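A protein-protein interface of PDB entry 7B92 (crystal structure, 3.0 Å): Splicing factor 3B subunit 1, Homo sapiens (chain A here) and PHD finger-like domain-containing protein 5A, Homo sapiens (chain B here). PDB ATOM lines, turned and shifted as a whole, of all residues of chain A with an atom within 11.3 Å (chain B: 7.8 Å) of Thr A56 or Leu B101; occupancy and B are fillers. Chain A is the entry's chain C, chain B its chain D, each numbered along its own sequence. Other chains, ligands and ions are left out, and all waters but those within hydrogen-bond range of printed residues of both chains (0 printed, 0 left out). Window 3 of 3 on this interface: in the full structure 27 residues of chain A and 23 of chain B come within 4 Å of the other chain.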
ATOM      1  N   ASN A  11      17.814  25.394 -21.735  1.00  0.00           N
ATOM      2  CA  ASN A  11      16.557  25.518 -21.007  1.00  0.00           C
ATOM      3  C   ASN A  11      16.809  25.638 -19.507  1.00  0.00           C
ATOM      4  O   ASN A  11      17.958  25.710 -19.066  1.00  0.00           O
ATOM      5  CB  ASN A  11      15.647  24.322 -21.297  1.00  0.00           C
ATOM      6  CG  ASN A  11      15.276  24.214 -22.765  1.00  0.00           C
ATOM      7  OD1 ASN A  11      15.138  25.223 -23.458  1.00  0.00           O
ATOM      8  ND2 ASN A  11      15.117  22.986 -23.246  1.00  0.00           N
ATOM      9  N   LEU A  12      15.730  25.656 -18.726  1.00  0.00           N
ATOM     10  CA  LEU A  12      15.885  25.795 -17.284  1.00  0.00           C
ATOM     11  C   LEU A  12      15.738  24.447 -16.590  1.00  0.00           C
ATOM     12  O   LEU A  12      14.844  23.664 -16.933  1.00  0.00           O
ATOM     13  CB  LEU A  12      14.855  26.771 -16.711  1.00  0.00           C
ATOM     14  CG  LEU A  12      15.152  28.270 -16.831  1.00  0.00           C
ATOM     15  CD1 LEU A  12      14.987  28.775 -18.263  1.00  0.00           C
ATOM     16  CD2 LEU A  12      14.275  29.063 -15.876  1.00  0.00           C
ATOM     17  N   PRO A  13      16.607  24.158 -15.615  1.00  0.00           N
ATOM     18  CA  PRO A  13      16.517  22.882 -14.890  1.00  0.00           C
ATOM     19  C   PRO A  13      15.244  22.743 -14.069  1.00  0.00           C
ATOM     20  O   PRO A  13      14.408  23.651 -14.033  1.00  0.00           O
ATOM     21  CB  PRO A  13      17.755  22.907 -13.984  1.00  0.00           C
ATOM     22  CG  PRO A  13      18.699  23.840 -14.656  1.00  0.00           C
ATOM     23  CD  PRO A  13      17.840  24.892 -15.289  1.00  0.00           C
ATOM     24  N   PHE A  14      15.100  21.604 -13.400  1.00  0.00           N
ATOM     25  CA  PHE A  14      13.917  21.345 -12.594  1.00  0.00           C
ATOM     26  C   PHE A  14      13.945  22.168 -11.310  1.00  0.00           C
ATOM     27  O   PHE A  14      15.005  22.438 -10.739  1.00  0.00           O
ATOM     28  CB  PHE A  14      13.821  19.855 -12.264  1.00  0.00           C
ATOM     29  CG  PHE A  14      12.573  19.475 -11.519  1.00  0.00           C
ATOM     30  CD1 PHE A  14      11.398  19.211 -12.200  1.00  0.00           C
ATOM     31  CD2 PHE A  14      12.578  19.379 -10.137  1.00  0.00           C
ATOM     32  CE1 PHE A  14      10.250  18.860 -11.518  1.00  0.00           C
ATOM     33  CE2 PHE A  14      11.434  19.030  -9.449  1.00  0.00           C
ATOM     34  CZ  PHE A  14      10.267  18.770 -10.140  1.00  0.00           C
ATOM     35  N   LYS A  47      19.909  33.379 -12.388  1.00  0.00           N
ATOM     36  CA  LYS A  47      19.909  32.256 -13.326  1.00  0.00           C
ATOM     37  C   LYS A  47      21.139  31.367 -13.144  1.00  0.00           C
ATOM     38  O   LYS A  47      21.038  30.128 -13.181  1.00  0.00           O
ATOM     39  CB  LYS A  47      19.835  32.786 -14.757  1.00  0.00           C
ATOM     40  CG  LYS A  47      19.686  31.725 -15.836  1.00  0.00           C
ATOM     41  CD  LYS A  47      19.965  32.330 -17.207  1.00  0.00           C
ATOM     42  CE  LYS A  47      18.724  32.335 -18.087  1.00  0.00           C
ATOM     43  NZ  LYS A  47      19.065  32.430 -19.534  1.00  0.00           N
ATOM     44  N   LEU A  48      22.313  31.980 -12.973  1.00  0.00           N
ATOM     45  CA  LEU A  48      23.537  31.209 -12.775  1.00  0.00           C
ATOM     46  C   LEU A  48      23.450  30.354 -11.518  1.00  0.00           C
ATOM     47  O   LEU A  48      23.911  29.206 -11.505  1.00  0.00           O
ATOM     48  CB  LEU A  48      24.747  32.146 -12.707  1.00  0.00           C
ATOM     49  CG  LEU A  48      25.516  32.482 -13.991  1.00  0.00           C
ATOM     50  CD1 LEU A  48      26.339  31.290 -14.442  1.00  0.00           C
ATOM     51  CD2 LEU A  48      24.598  32.949 -15.115  1.00  0.00           C
ATOM     52  N   LEU A  49      22.852  30.889 -10.449  1.00  0.00           N
ATOM     53  CA  LEU A  49      22.730  30.097  -9.228  1.00  0.00           C
ATOM     54  C   LEU A  49      21.762  28.932  -9.403  1.00  0.00           C
ATOM     55  O   LEU A  49      21.964  27.871  -8.803  1.00  0.00           O
ATOM     56  CB  LEU A  49      22.300  30.973  -8.056  1.00  0.00           C
ATOM     57  CG  LEU A  49      23.369  31.934  -7.540  1.00  0.00           C
ATOM     58  CD1 LEU A  49      22.941  32.545  -6.221  1.00  0.00           C
ATOM     59  CD2 LEU A  49      24.702  31.226  -7.392  1.00  0.00           C
ATOM     60  N   LEU A  50      20.710  29.106 -10.205  1.00  0.00           N
ATOM     61  CA  LEU A  50      19.832  27.981 -10.508  1.00  0.00           C
ATOM     62  C   LEU A  50      20.598  26.889 -11.243  1.00  0.00           C
ATOM     63  O   LEU A  50      20.479  25.702 -10.915  1.00  0.00           O
ATOM     64  CB  LEU A  50      18.623  28.452 -11.325  1.00  0.00           C
ATOM     65  CG  LEU A  50      17.333  27.616 -11.352  1.00  0.00           C
ATOM     66  CD1 LEU A  50      17.488  26.280 -12.063  1.00  0.00           C
ATOM     67  CD2 LEU A  50      16.832  27.390  -9.943  1.00  0.00           C
ATOM     68  N   LYS A  51      21.400  27.271 -12.240  1.00  0.00           N
ATOM     69  CA  LYS A  51      22.190  26.254 -12.935  1.00  0.00           C
ATOM     70  C   LYS A  51      23.207  25.592 -12.008  1.00  0.00           C
ATOM     71  O   LYS A  51      23.513  24.405 -12.173  1.00  0.00           O
ATOM     72  CB  LYS A  51      22.889  26.843 -14.161  1.00  0.00           C
ATOM     73  CG  LYS A  51      21.944  27.301 -15.259  1.00  0.00           C
ATOM     74  CD  LYS A  51      22.713  27.723 -16.499  1.00  0.00           C
ATOM     75  CE  LYS A  51      23.436  26.538 -17.131  1.00  0.00           C
ATOM     76  NZ  LYS A  51      22.503  25.474 -17.605  1.00  0.00           N
ATOM     77  N   ILE A  52      23.733  26.329 -11.027  1.00  0.00           N
ATOM     78  CA  ILE A  52      24.695  25.741 -10.094  1.00  0.00           C
ATOM     79  C   ILE A  52      24.009  24.741  -9.168  1.00  0.00           C
ATOM     80  O   ILE A  52      24.437  23.588  -9.047  1.00  0.00           O
ATOM     81  CB  ILE A  52      25.413  26.839  -9.288  1.00  0.00           C
ATOM     82  CG1 ILE A  52      26.397  27.609 -10.168  1.00  0.00           C
ATOM     83  CG2 ILE A  52      26.127  26.234  -8.087  1.00  0.00           C
ATOM     84  CD1 ILE A  52      27.157  28.692  -9.432  1.00  0.00           C
ATOM     85  N   LYS A  53      22.941  25.173  -8.497  1.00  0.00           N
ATOM     86  CA  LYS A  53      22.312  24.355  -7.463  1.00  0.00           C
ATOM     87  C   LYS A  53      21.695  23.091  -8.050  1.00  0.00           C
ATOM     88  O   LYS A  53      22.065  21.973  -7.674  1.00  0.00           O
ATOM     89  CB  LYS A  53      21.262  25.186  -6.723  1.00  0.00           C
ATOM     90  CG  LYS A  53      20.515  24.442  -5.636  1.00  0.00           C
ATOM     91  CD  LYS A  53      19.573  25.380  -4.903  1.00  0.00           C
ATOM     92  CE  LYS A  53      18.622  24.621  -3.996  1.00  0.00           C
ATOM     93  NZ  LYS A  53      17.741  23.701  -4.767  1.00  0.00           N
ATOM     94  N   ASN A  54      20.750  23.244  -8.970  1.00  0.00           N
ATOM     95  CA  ASN A  54      20.090  22.115  -9.620  1.00  0.00           C
ATOM     96  C   ASN A  54      20.582  22.055 -11.062  1.00  0.00           C
ATOM     97  O   ASN A  54      20.170  22.862 -11.900  1.00  0.00           O
ATOM     98  CB  ASN A  54      18.572  22.260  -9.552  1.00  0.00           C
ATOM     99  CG  ASN A  54      18.076  22.535  -8.145  1.00  0.00           C
ATOM    100  OD1 ASN A  54      17.998  23.687  -7.720  1.00  0.00           O
ATOM    101  ND2 ASN A  54      17.734  21.476  -7.417  1.00  0.00           N
ATOM    102  N   GLY A  55      21.464  21.107 -11.351  1.00  0.00           N
ATOM    103  CA  GLY A  55      21.999  20.986 -12.694  1.00  0.00           C
ATOM    104  C   GLY A  55      22.961  19.821 -12.797  1.00  0.00           C
ATOM    105  O   GLY A  55      23.472  19.313 -11.793  1.00  0.00           O
ATOM    106  N   THR A  56      23.195  19.410 -14.041  1.00  0.00           N
ATOM    107  CA  THR A  56      24.123  18.333 -14.328  1.00  0.00           C
ATOM    108  C   THR A  56      25.559  18.797 -14.084  1.00  0.00           C
ATOM    109  O   THR A  56      25.826  19.999 -14.021  1.00  0.00           O
ATOM    110  CB  THR A  56      23.951  17.867 -15.773  1.00  0.00           C
ATOM    111  OG1 THR A  56      24.266  18.942 -16.666  1.00  0.00           O
ATOM    112  CG2 THR A  56      22.518  17.422 -16.017  1.00  0.00           C
ATOM    113  N   PRO A  57      26.496  17.862 -13.924  1.00  0.00           N
ATOM    114  CA  PRO A  57      27.901  18.239 -13.693  1.00  0.00           C
ATOM    115  C   PRO A  57      28.441  19.174 -14.765  1.00  0.00           C
ATOM    116  O   PRO A  57      29.147  20.138 -14.429  1.00  0.00           O
ATOM    117  CB  PRO A  57      28.632  16.887 -13.695  1.00  0.00           C
ATOM    118  CG  PRO A  57      27.612  15.933 -13.191  1.00  0.00           C
ATOM    119  CD  PRO A  57      26.279  16.418 -13.711  1.00  0.00           C
ATOM    120  N   PRO A  58      28.160  18.944 -16.062  1.00  0.00           N
ATOM    121  CA  PRO A  58      28.600  19.945 -17.052  1.00  0.00           C
ATOM    122  C   PRO A  58      27.980  21.315 -16.833  1.00  0.00           C
ATOM    123  O   PRO A  58      28.692  22.330 -16.892  1.00  0.00           O
ATOM    124  CB  PRO A  58      28.178  19.326 -18.394  1.00  0.00           C
ATOM    125  CG  PRO A  58      27.157  18.308 -18.050  1.00  0.00           C
ATOM    126  CD  PRO A  58      27.586  17.763 -16.736  1.00  0.00           C
ATOM    127  N   MET A  59      26.667  21.371 -16.579  1.00  0.00           N
ATOM    128  CA  MET A  59      26.022  22.640 -16.251  1.00  0.00           C
ATOM    129  C   MET A  59      26.660  23.285 -15.028  1.00  0.00           C
ATOM    130  O   MET A  59      26.901  24.497 -15.012  1.00  0.00           O
ATOM    131  CB  MET A  59      24.527  22.428 -16.006  1.00  0.00           C
ATOM    132  CG  MET A  59      23.721  22.035 -17.227  1.00  0.00           C
ATOM    133  SD  MET A  59      21.983  21.773 -16.811  1.00  0.00           S
ATOM    134  CE  MET A  59      21.329  21.246 -18.395  1.00  0.00           C
ATOM    135  N   ARG A  60      26.941  22.487 -13.994  1.00  0.00           N
ATOM    136  CA  ARG A  60      27.508  23.030 -12.765  1.00  0.00           C
ATOM    137  C   ARG A  60      28.892  23.620 -13.007  1.00  0.00           C
ATOM    138  O   ARG A  60      29.193  24.729 -12.552  1.00  0.00           O
ATOM    139  CB  ARG A  60      27.561  21.947 -11.687  1.00  0.00           C
ATOM    140  CG  ARG A  60      26.197  21.520 -11.163  1.00  0.00           C
ATOM    141  CD  ARG A  60      26.331  20.552  -9.997  1.00  0.00           C
ATOM    142  NE  ARG A  60      26.871  19.259 -10.408  1.00  0.00           N
ATOM    143  CZ  ARG A  60      27.532  18.436  -9.600  1.00  0.00           C
ATOM    144  NH1 ARG A  60      27.749  18.776  -8.338  1.00  0.00           N
ATOM    145  NH2 ARG A  60      27.985  17.277 -10.055  1.00  0.00           N
ATOM    146  N   LYS A  61      29.752  22.892 -13.728  1.00  0.00           N
ATOM    147  CA  LYS A  61      31.098  23.394 -13.990  1.00  0.00           C
ATOM    148  C   LYS A  61      31.066  24.643 -14.864  1.00  0.00           C
ATOM    149  O   LYS A  61      31.799  25.609 -14.604  1.00  0.00           O
ATOM    150  CB  LYS A  61      31.953  22.306 -14.642  1.00  0.00           C
ATOM    151  CG  LYS A  61      33.350  22.778 -15.029  1.00  0.00           C
ATOM    152  CD  LYS A  61      34.181  21.669 -15.661  1.00  0.00           C
ATOM    153  CE  LYS A  61      34.495  20.566 -14.663  1.00  0.00           C
ATOM    154  NZ  LYS A  61      35.407  19.539 -15.241  1.00  0.00           N
ATOM    155  N   ALA A  62      30.224  24.646 -15.904  1.00  0.00           N
ATOM    156  CA  ALA A  62      30.129  25.819 -16.767  1.00  0.00           C
ATOM    157  C   ALA A  62      29.616  27.028 -15.995  1.00  0.00           C
ATOM    158  O   ALA A  62      30.122  28.145 -16.167  1.00  0.00           O
ATOM    159  CB  ALA A  62      29.226  25.519 -17.961  1.00  0.00           C
ATOM    160  N   ALA A  63      28.623  26.824 -15.126  1.00  0.00           N
ATOM    161  CA  ALA A  63      28.092  27.932 -14.343  1.00  0.00           C
ATOM    162  C   ALA A  63      29.107  28.422 -13.317  1.00  0.00           C
ATOM    163  O   ALA A  63      29.185  29.623 -13.045  1.00  0.00           O
ATOM    164  CB  ALA A  63      26.789  27.514 -13.665  1.00  0.00           C
ATOM    165  N   LEU A  64      29.897  27.512 -12.743  1.00  0.00           N
ATOM    166  CA  LEU A  64      30.970  27.924 -11.842  1.00  0.00           C
ATOM    167  C   LEU A  64      31.989  28.793 -12.567  1.00  0.00           C
ATOM    168  O   LEU A  64      32.395  29.846 -12.062  1.00  0.00           O
ATOM    169  CB  LEU A  64      31.652  26.696 -11.237  1.00  0.00           C
ATOM    170  CG  LEU A  64      31.103  26.167  -9.915  1.00  0.00           C
ATOM    171  CD1 LEU A  64      31.862  24.920  -9.486  1.00  0.00           C
ATOM    172  CD2 LEU A  64      31.196  27.242  -8.849  1.00  0.00           C
ATOM    173  N   ARG A  65      32.415  28.364 -13.758  1.00  0.00           N
ATOM    174  CA  ARG A  65      33.369  29.160 -14.523  1.00  0.00           C
ATOM    175  C   ARG A  65      32.785  30.523 -14.882  1.00  0.00           C
ATOM    176  O   ARG A  65      33.470  31.549 -14.781  1.00  0.00           O
ATOM    177  CB  ARG A  65      33.793  28.403 -15.782  1.00  0.00           C
ATOM    178  CG  ARG A  65      34.924  29.060 -16.561  1.00  0.00           C
ATOM    179  CD  ARG A  65      35.403  28.162 -17.690  1.00  0.00           C
ATOM    180  NE  ARG A  65      35.872  26.871 -17.194  1.00  0.00           N
ATOM    181  CZ  ARG A  65      36.308  25.883 -17.969  1.00  0.00           C
ATOM    182  NH1 ARG A  65      36.339  26.032 -19.287  1.00  0.00           N
ATOM    183  NH2 ARG A  65      36.714  24.742 -17.427  1.00  0.00           N
ATOM    184  N   LEU A  99      27.832  22.971  -2.370  1.00  0.00           N
ATOM    185  CA  LEU A  99      28.009  23.676  -3.638  1.00  0.00           C
ATOM    186  C   LEU A  99      28.010  25.186  -3.430  1.00  0.00           C
ATOM    187  O   LEU A  99      28.806  25.908  -4.046  1.00  0.00           O
ATOM    188  CB  LEU A  99      26.914  23.277  -4.626  1.00  0.00           C
ATOM    189  CG  LEU A  99      27.237  22.155  -5.615  1.00  0.00           C
ATOM    190  CD1 LEU A  99      27.566  20.855  -4.893  1.00  0.00           C
ATOM    191  CD2 LEU A  99      26.087  21.955  -6.585  1.00  0.00           C
ATOM    192  N   PRO B  16      21.095   5.906 -19.935  1.00  0.00           N
ATOM    193  CA  PRO B  16      21.932   6.486 -18.877  1.00  0.00           C
ATOM    194  C   PRO B  16      23.390   6.639 -19.307  1.00  0.00           C
ATOM    195  O   PRO B  16      24.005   5.666 -19.748  1.00  0.00           O
ATOM    196  CB  PRO B  16      21.798   5.477 -17.733  1.00  0.00           C
ATOM    197  CG  PRO B  16      21.475   4.185 -18.407  1.00  0.00           C
ATOM    198  CD  PRO B  16      20.631   4.549 -19.594  1.00  0.00           C
ATOM    199  N   ASP B  17      23.936   7.849 -19.176  1.00  0.00           N
ATOM    200  CA  ASP B  17      25.298   8.160 -19.612  1.00  0.00           C
ATOM    201  C   ASP B  17      26.175   8.357 -18.379  1.00  0.00           C
ATOM    202  O   ASP B  17      26.182   9.432 -17.772  1.00  0.00           O
ATOM    203  CB  ASP B  17      25.311   9.391 -20.513  1.00  0.00           C
ATOM    204  CG  ASP B  17      26.657   9.613 -21.175  1.00  0.00           C
ATOM    205  OD1 ASP B  17      27.097   8.729 -21.943  1.00  0.00           O
ATOM    206  OD2 ASP B  17      27.269  10.674 -20.933  1.00  0.00           O
ATOM    207  N   LEU B  18      26.924   7.318 -18.021  1.00  0.00           N
ATOM    208  CA  LEU B  18      27.775   7.305 -16.842  1.00  0.00           C
ATOM    209  C   LEU B  18      29.239   7.357 -17.260  1.00  0.00           C
ATOM    210  O   LEU B  18      29.587   7.135 -18.422  1.00  0.00           O
ATOM    211  CB  LEU B  18      27.507   6.056 -15.990  1.00  0.00           C
ATOM    212  CG  LEU B  18      26.190   5.962 -15.211  1.00  0.00           C
ATOM    213  CD1 LEU B  18      25.000   5.717 -16.122  1.00  0.00           C
ATOM    214  CD2 LEU B  18      26.271   4.867 -14.160  1.00  0.00           C
ATOM    215  N   ILE B  19      30.102   7.656 -16.289  1.00  0.00           N
ATOM    216  CA  ILE B  19      31.538   7.718 -16.548  1.00  0.00           C
ATOM    217  C   ILE B  19      32.294   7.614 -15.227  1.00  0.00           C
ATOM    218  O   ILE B  19      31.685   7.549 -14.155  1.00  0.00           O
ATOM    219  CB  ILE B  19      31.904   9.004 -17.319  1.00  0.00           C
ATOM    220  CG1 ILE B  19      33.188   8.808 -18.137  1.00  0.00           C
ATOM    221  CG2 ILE B  19      32.026  10.191 -16.374  1.00  0.00           C
ATOM    222  CD1 ILE B  19      33.133   7.639 -19.111  1.00  0.00           C
ATOM    223  N   PHE B  20      33.620   7.557 -15.295  1.00  0.00           N
ATOM    224  CA  PHE B  20      34.449   7.573 -14.102  1.00  0.00           C
ATOM    225  C   PHE B  20      34.826   9.006 -13.744  1.00  0.00           C
ATOM    226  O   PHE B  20      34.932   9.877 -14.611  1.00  0.00           O
ATOM    227  CB  PHE B  20      35.719   6.742 -14.298  1.00  0.00           C
ATOM    228  CG  PHE B  20      35.472   5.263 -14.441  1.00  0.00           C
ATOM    229  CD1 PHE B  20      35.408   4.445 -13.326  1.00  0.00           C
ATOM    230  CD2 PHE B  20      35.325   4.689 -15.693  1.00  0.00           C
ATOM    231  CE1 PHE B  20      35.190   3.084 -13.454  1.00  0.00           C
ATOM    232  CE2 PHE B  20      35.108   3.328 -15.828  1.00  0.00           C
ATOM    233  CZ  PHE B  20      35.040   2.525 -14.704  1.00  0.00           C
ATOM    234  N   ILE B  98      32.020   6.123  -9.956  1.00  0.00           N
ATOM    235  CA  ILE B  98      31.056   6.209 -11.048  1.00  0.00           C
ATOM    236  C   ILE B  98      30.198   7.449 -10.835  1.00  0.00           C
ATOM    237  O   ILE B  98      29.600   7.625  -9.768  1.00  0.00           O
ATOM    238  CB  ILE B  98      30.188   4.945 -11.123  1.00  0.00           C
ATOM    239  CG1 ILE B  98      31.033   3.686 -10.901  1.00  0.00           C
ATOM    240  CG2 ILE B  98      29.484   4.875 -12.464  1.00  0.00           C
ATOM    241  CD1 ILE B  98      31.992   3.375 -12.027  1.00  0.00           C
ATOM    242  N   VAL B  99      30.141   8.315 -11.843  1.00  0.00           N
ATOM    243  CA  VAL B  99      29.316   9.515 -11.806  1.00  0.00           C
ATOM    244  C   VAL B  99      28.390   9.515 -13.015  1.00  0.00           C
ATOM    245  O   VAL B  99      28.784   9.116 -14.119  1.00  0.00           O
ATOM    246  CB  VAL B  99      30.166  10.804 -11.758  1.00  0.00           C
ATOM    247  CG1 VAL B  99      31.017  10.824 -10.504  1.00  0.00           C
ATOM    248  CG2 VAL B  99      31.042  10.926 -12.989  1.00  0.00           C
ATOM    249  N   ASN B 100      27.154   9.960 -12.801  1.00  0.00           N
ATOM    250  CA  ASN B 100      26.135  10.021 -13.840  1.00  0.00           C
ATOM    251  C   ASN B 100      25.933  11.475 -14.247  1.00  0.00           C
ATOM    252  O   ASN B 100      25.482  12.293 -13.438  1.00  0.00           O
ATOM    253  CB  ASN B 100      24.821   9.409 -13.353  1.00  0.00           C
ATOM    254  CG  ASN B 100      23.717   9.488 -14.390  1.00  0.00           C
ATOM    255  OD1 ASN B 100      23.976   9.606 -15.588  1.00  0.00           O
ATOM    256  ND2 ASN B 100      22.473   9.420 -13.931  1.00  0.00           N
ATOM    257  N   LEU B 101      26.260  11.789 -15.498  1.00  0.00           N
ATOM    258  CA  LEU B 101      26.143  13.141 -16.041  1.00  0.00           C
ATOM    259  C   LEU B 101      24.698  13.578 -16.264  1.00  0.00           C
ATOM    260  O   LEU B 101      24.488  14.658 -16.834  1.00  0.00           O
ATOM    261  CB  LEU B 101      26.923  13.244 -17.352  1.00  0.00           C
ATOM    262  CG  LEU B 101      28.422  13.544 -17.266  1.00  0.00           C
ATOM    263  CD1 LEU B 101      29.174  12.405 -16.607  1.00  0.00           C
ATOM    264  CD2 LEU B 101      28.990  13.824 -18.647  1.00  0.00           C
ATOM    265  N   GLY B 102      23.708  12.792 -15.848  1.00  0.00           N
ATOM    266  CA  GLY B 102      22.319  13.157 -16.036  1.00  0.00           C
ATOM    267  C   GLY B 102      21.570  13.307 -14.729  1.00  0.00           C
ATOM    268  O   GLY B 102      20.390  12.955 -14.638  1.00  0.00           O
ATOM    269  N   SER B 103      22.250  13.825 -13.709  1.00  0.00           N
ATOM    270  CA  SER B 103      21.635  14.047 -12.408  1.00  0.00           C
ATOM    271  C   SER B 103      22.474  15.060 -11.642  1.00  0.00           C
ATOM    272  O   SER B 103      23.578  15.423 -12.054  1.00  0.00           O
ATOM    273  CB  SER B 103      21.496  12.738 -11.624  1.00  0.00           C
ATOM    274  OG  SER B 103      22.745  12.085 -11.496  1.00  0.00           O
ATOM    275  N   SER B 104      21.929  15.517 -10.516  1.00  0.00           N
ATOM    276  CA  SER B 104      22.581  16.491  -9.661  1.00  0.00           C
ATOM    277  C   SER B 104      23.014  15.823  -8.354  1.00  0.00           C
ATOM    278  O   SER B 104      23.164  14.594  -8.289  1.00  0.00           O
ATOM    279  CB  SER B 104      21.638  17.675  -9.436  1.00  0.00           C
ATOM    280  OG  SER B 104      22.260  18.670  -8.641  1.00  0.00           O
ATOM    281  N   LYS B 105      23.214  16.633  -7.314  1.00  0.00           N
ATOM    282  CA  LYS B 105      23.633  16.130  -6.012  1.00  0.00           C
ATOM    283  C   LYS B 105      22.466  15.768  -5.102  1.00  0.00           C
ATOM    284  O   LYS B 105      22.692  15.197  -4.030  1.00  0.00           O
ATOM    285  CB  LYS B 105      24.524  17.158  -5.306  1.00  0.00           C
ATOM    286  CG  LYS B 105      25.774  17.534  -6.080  1.00  0.00           C
ATOM    287  CD  LYS B 105      26.611  16.304  -6.405  1.00  0.00           C
ATOM    288  CE  LYS B 105      27.157  15.642  -5.147  1.00  0.00           C
ATOM    289  NZ  LYS B 105      27.869  14.371  -5.461  1.00  0.00           N
ATOM    290  N   ASP B 107      19.489  14.163  -6.423  1.00  0.00           N
ATOM    291  CA  ASP B 107      18.746  13.038  -6.972  1.00  0.00           C
ATOM    292  C   ASP B 107      19.188  11.743  -6.303  1.00  0.00           C
ATOM    293  O   ASP B 107      20.384  11.441  -6.243  1.00  0.00           O
ATOM    294  CB  ASP B 107      18.951  12.958  -8.485  1.00  0.00           C
ATOM    295  CG  ASP B 107      18.567  14.246  -9.193  1.00  0.00           C
ATOM    296  OD1 ASP B 107      17.765  15.019  -8.627  1.00  0.00           O
ATOM    297  OD2 ASP B 107      19.062  14.485 -10.315  1.00  0.00           O
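The backbone carbonyl oxygen of Lys A53 lies within hydrogen-bond range of the side-chain hydroxyl of Ser B104 (3.4 Å).
O of Gly A55 sits close to OG of Ser B104 (3.4 Å).
OD1 of Asn A54 lies within hydrogen-bond range of NZ of Lys A53 (3.0 Å).
OG1 of Thr A56 lies close to N of Met A59 (3.4 Å).
O of Asp B17 lies within hydrogen-bond range of N of Leu B101 (3.3 Å).
The backbone carbonyl oxygen (O) of Asn B100 sits at hydrogen-bond distance from the side-chain hydroxyl (OG) of Ser B103, at 3.4 Å.
OD2 of Asp B107 lies within hydrogen-bond range of N of Ser B104 (3.1 Å).
Among the printed residues, merely in contact across the chains: Arg A60 with Lys B105, Pro A57 with Ser B103, Thr A56 with Leu B101, Thr A56 with Ser B103, Gly A55 with Ser B103 and Leu A99 with Lys B105.
Thr A56 touches just these residues of chain B: Leu B101 (3.4 Å) and Ser B103 (3.7 Å).
Printed residues of chain A within 4 Å of Leu B101: Thr A56.
Of chain B, only Ser B103 (3.9 Å) and Ser B104 (3.4 Å) come within 4 Å of Gly A55.
No residue of chain A comes within 4 Å of Leu B18.
No residue of chain A comes within 4 Å of Ile B19.
Val B99 touches none of the printed residues of chain A.
Asn B100 touches none of the printed residues of chain A.
Ser B104 touches just these residues of chain A: Lys A53 (3.4 Å) and Gly A55 (3.4 Å).
Of the printed residues of chain B, Pro A57 touches Ser B103.
Printed residues of chain A within 4 Å of Lys B105: Arg A60 and Leu A99.
Ile A52 touches none of the printed residues of chain B.
Of the 24 printed residues of chain A, 6 touch a printed residue of chain B.
Along chain A the printed residues that touch a printed residue of chain B span positions 53 to 99.
Printed residues of chain B that touch a printed residue of chain A: Leu B101, Ser B103, Ser B104 and Lys B105.
Along chain B the printed residues that touch a printed residue of chain A span positions 101 to 105.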
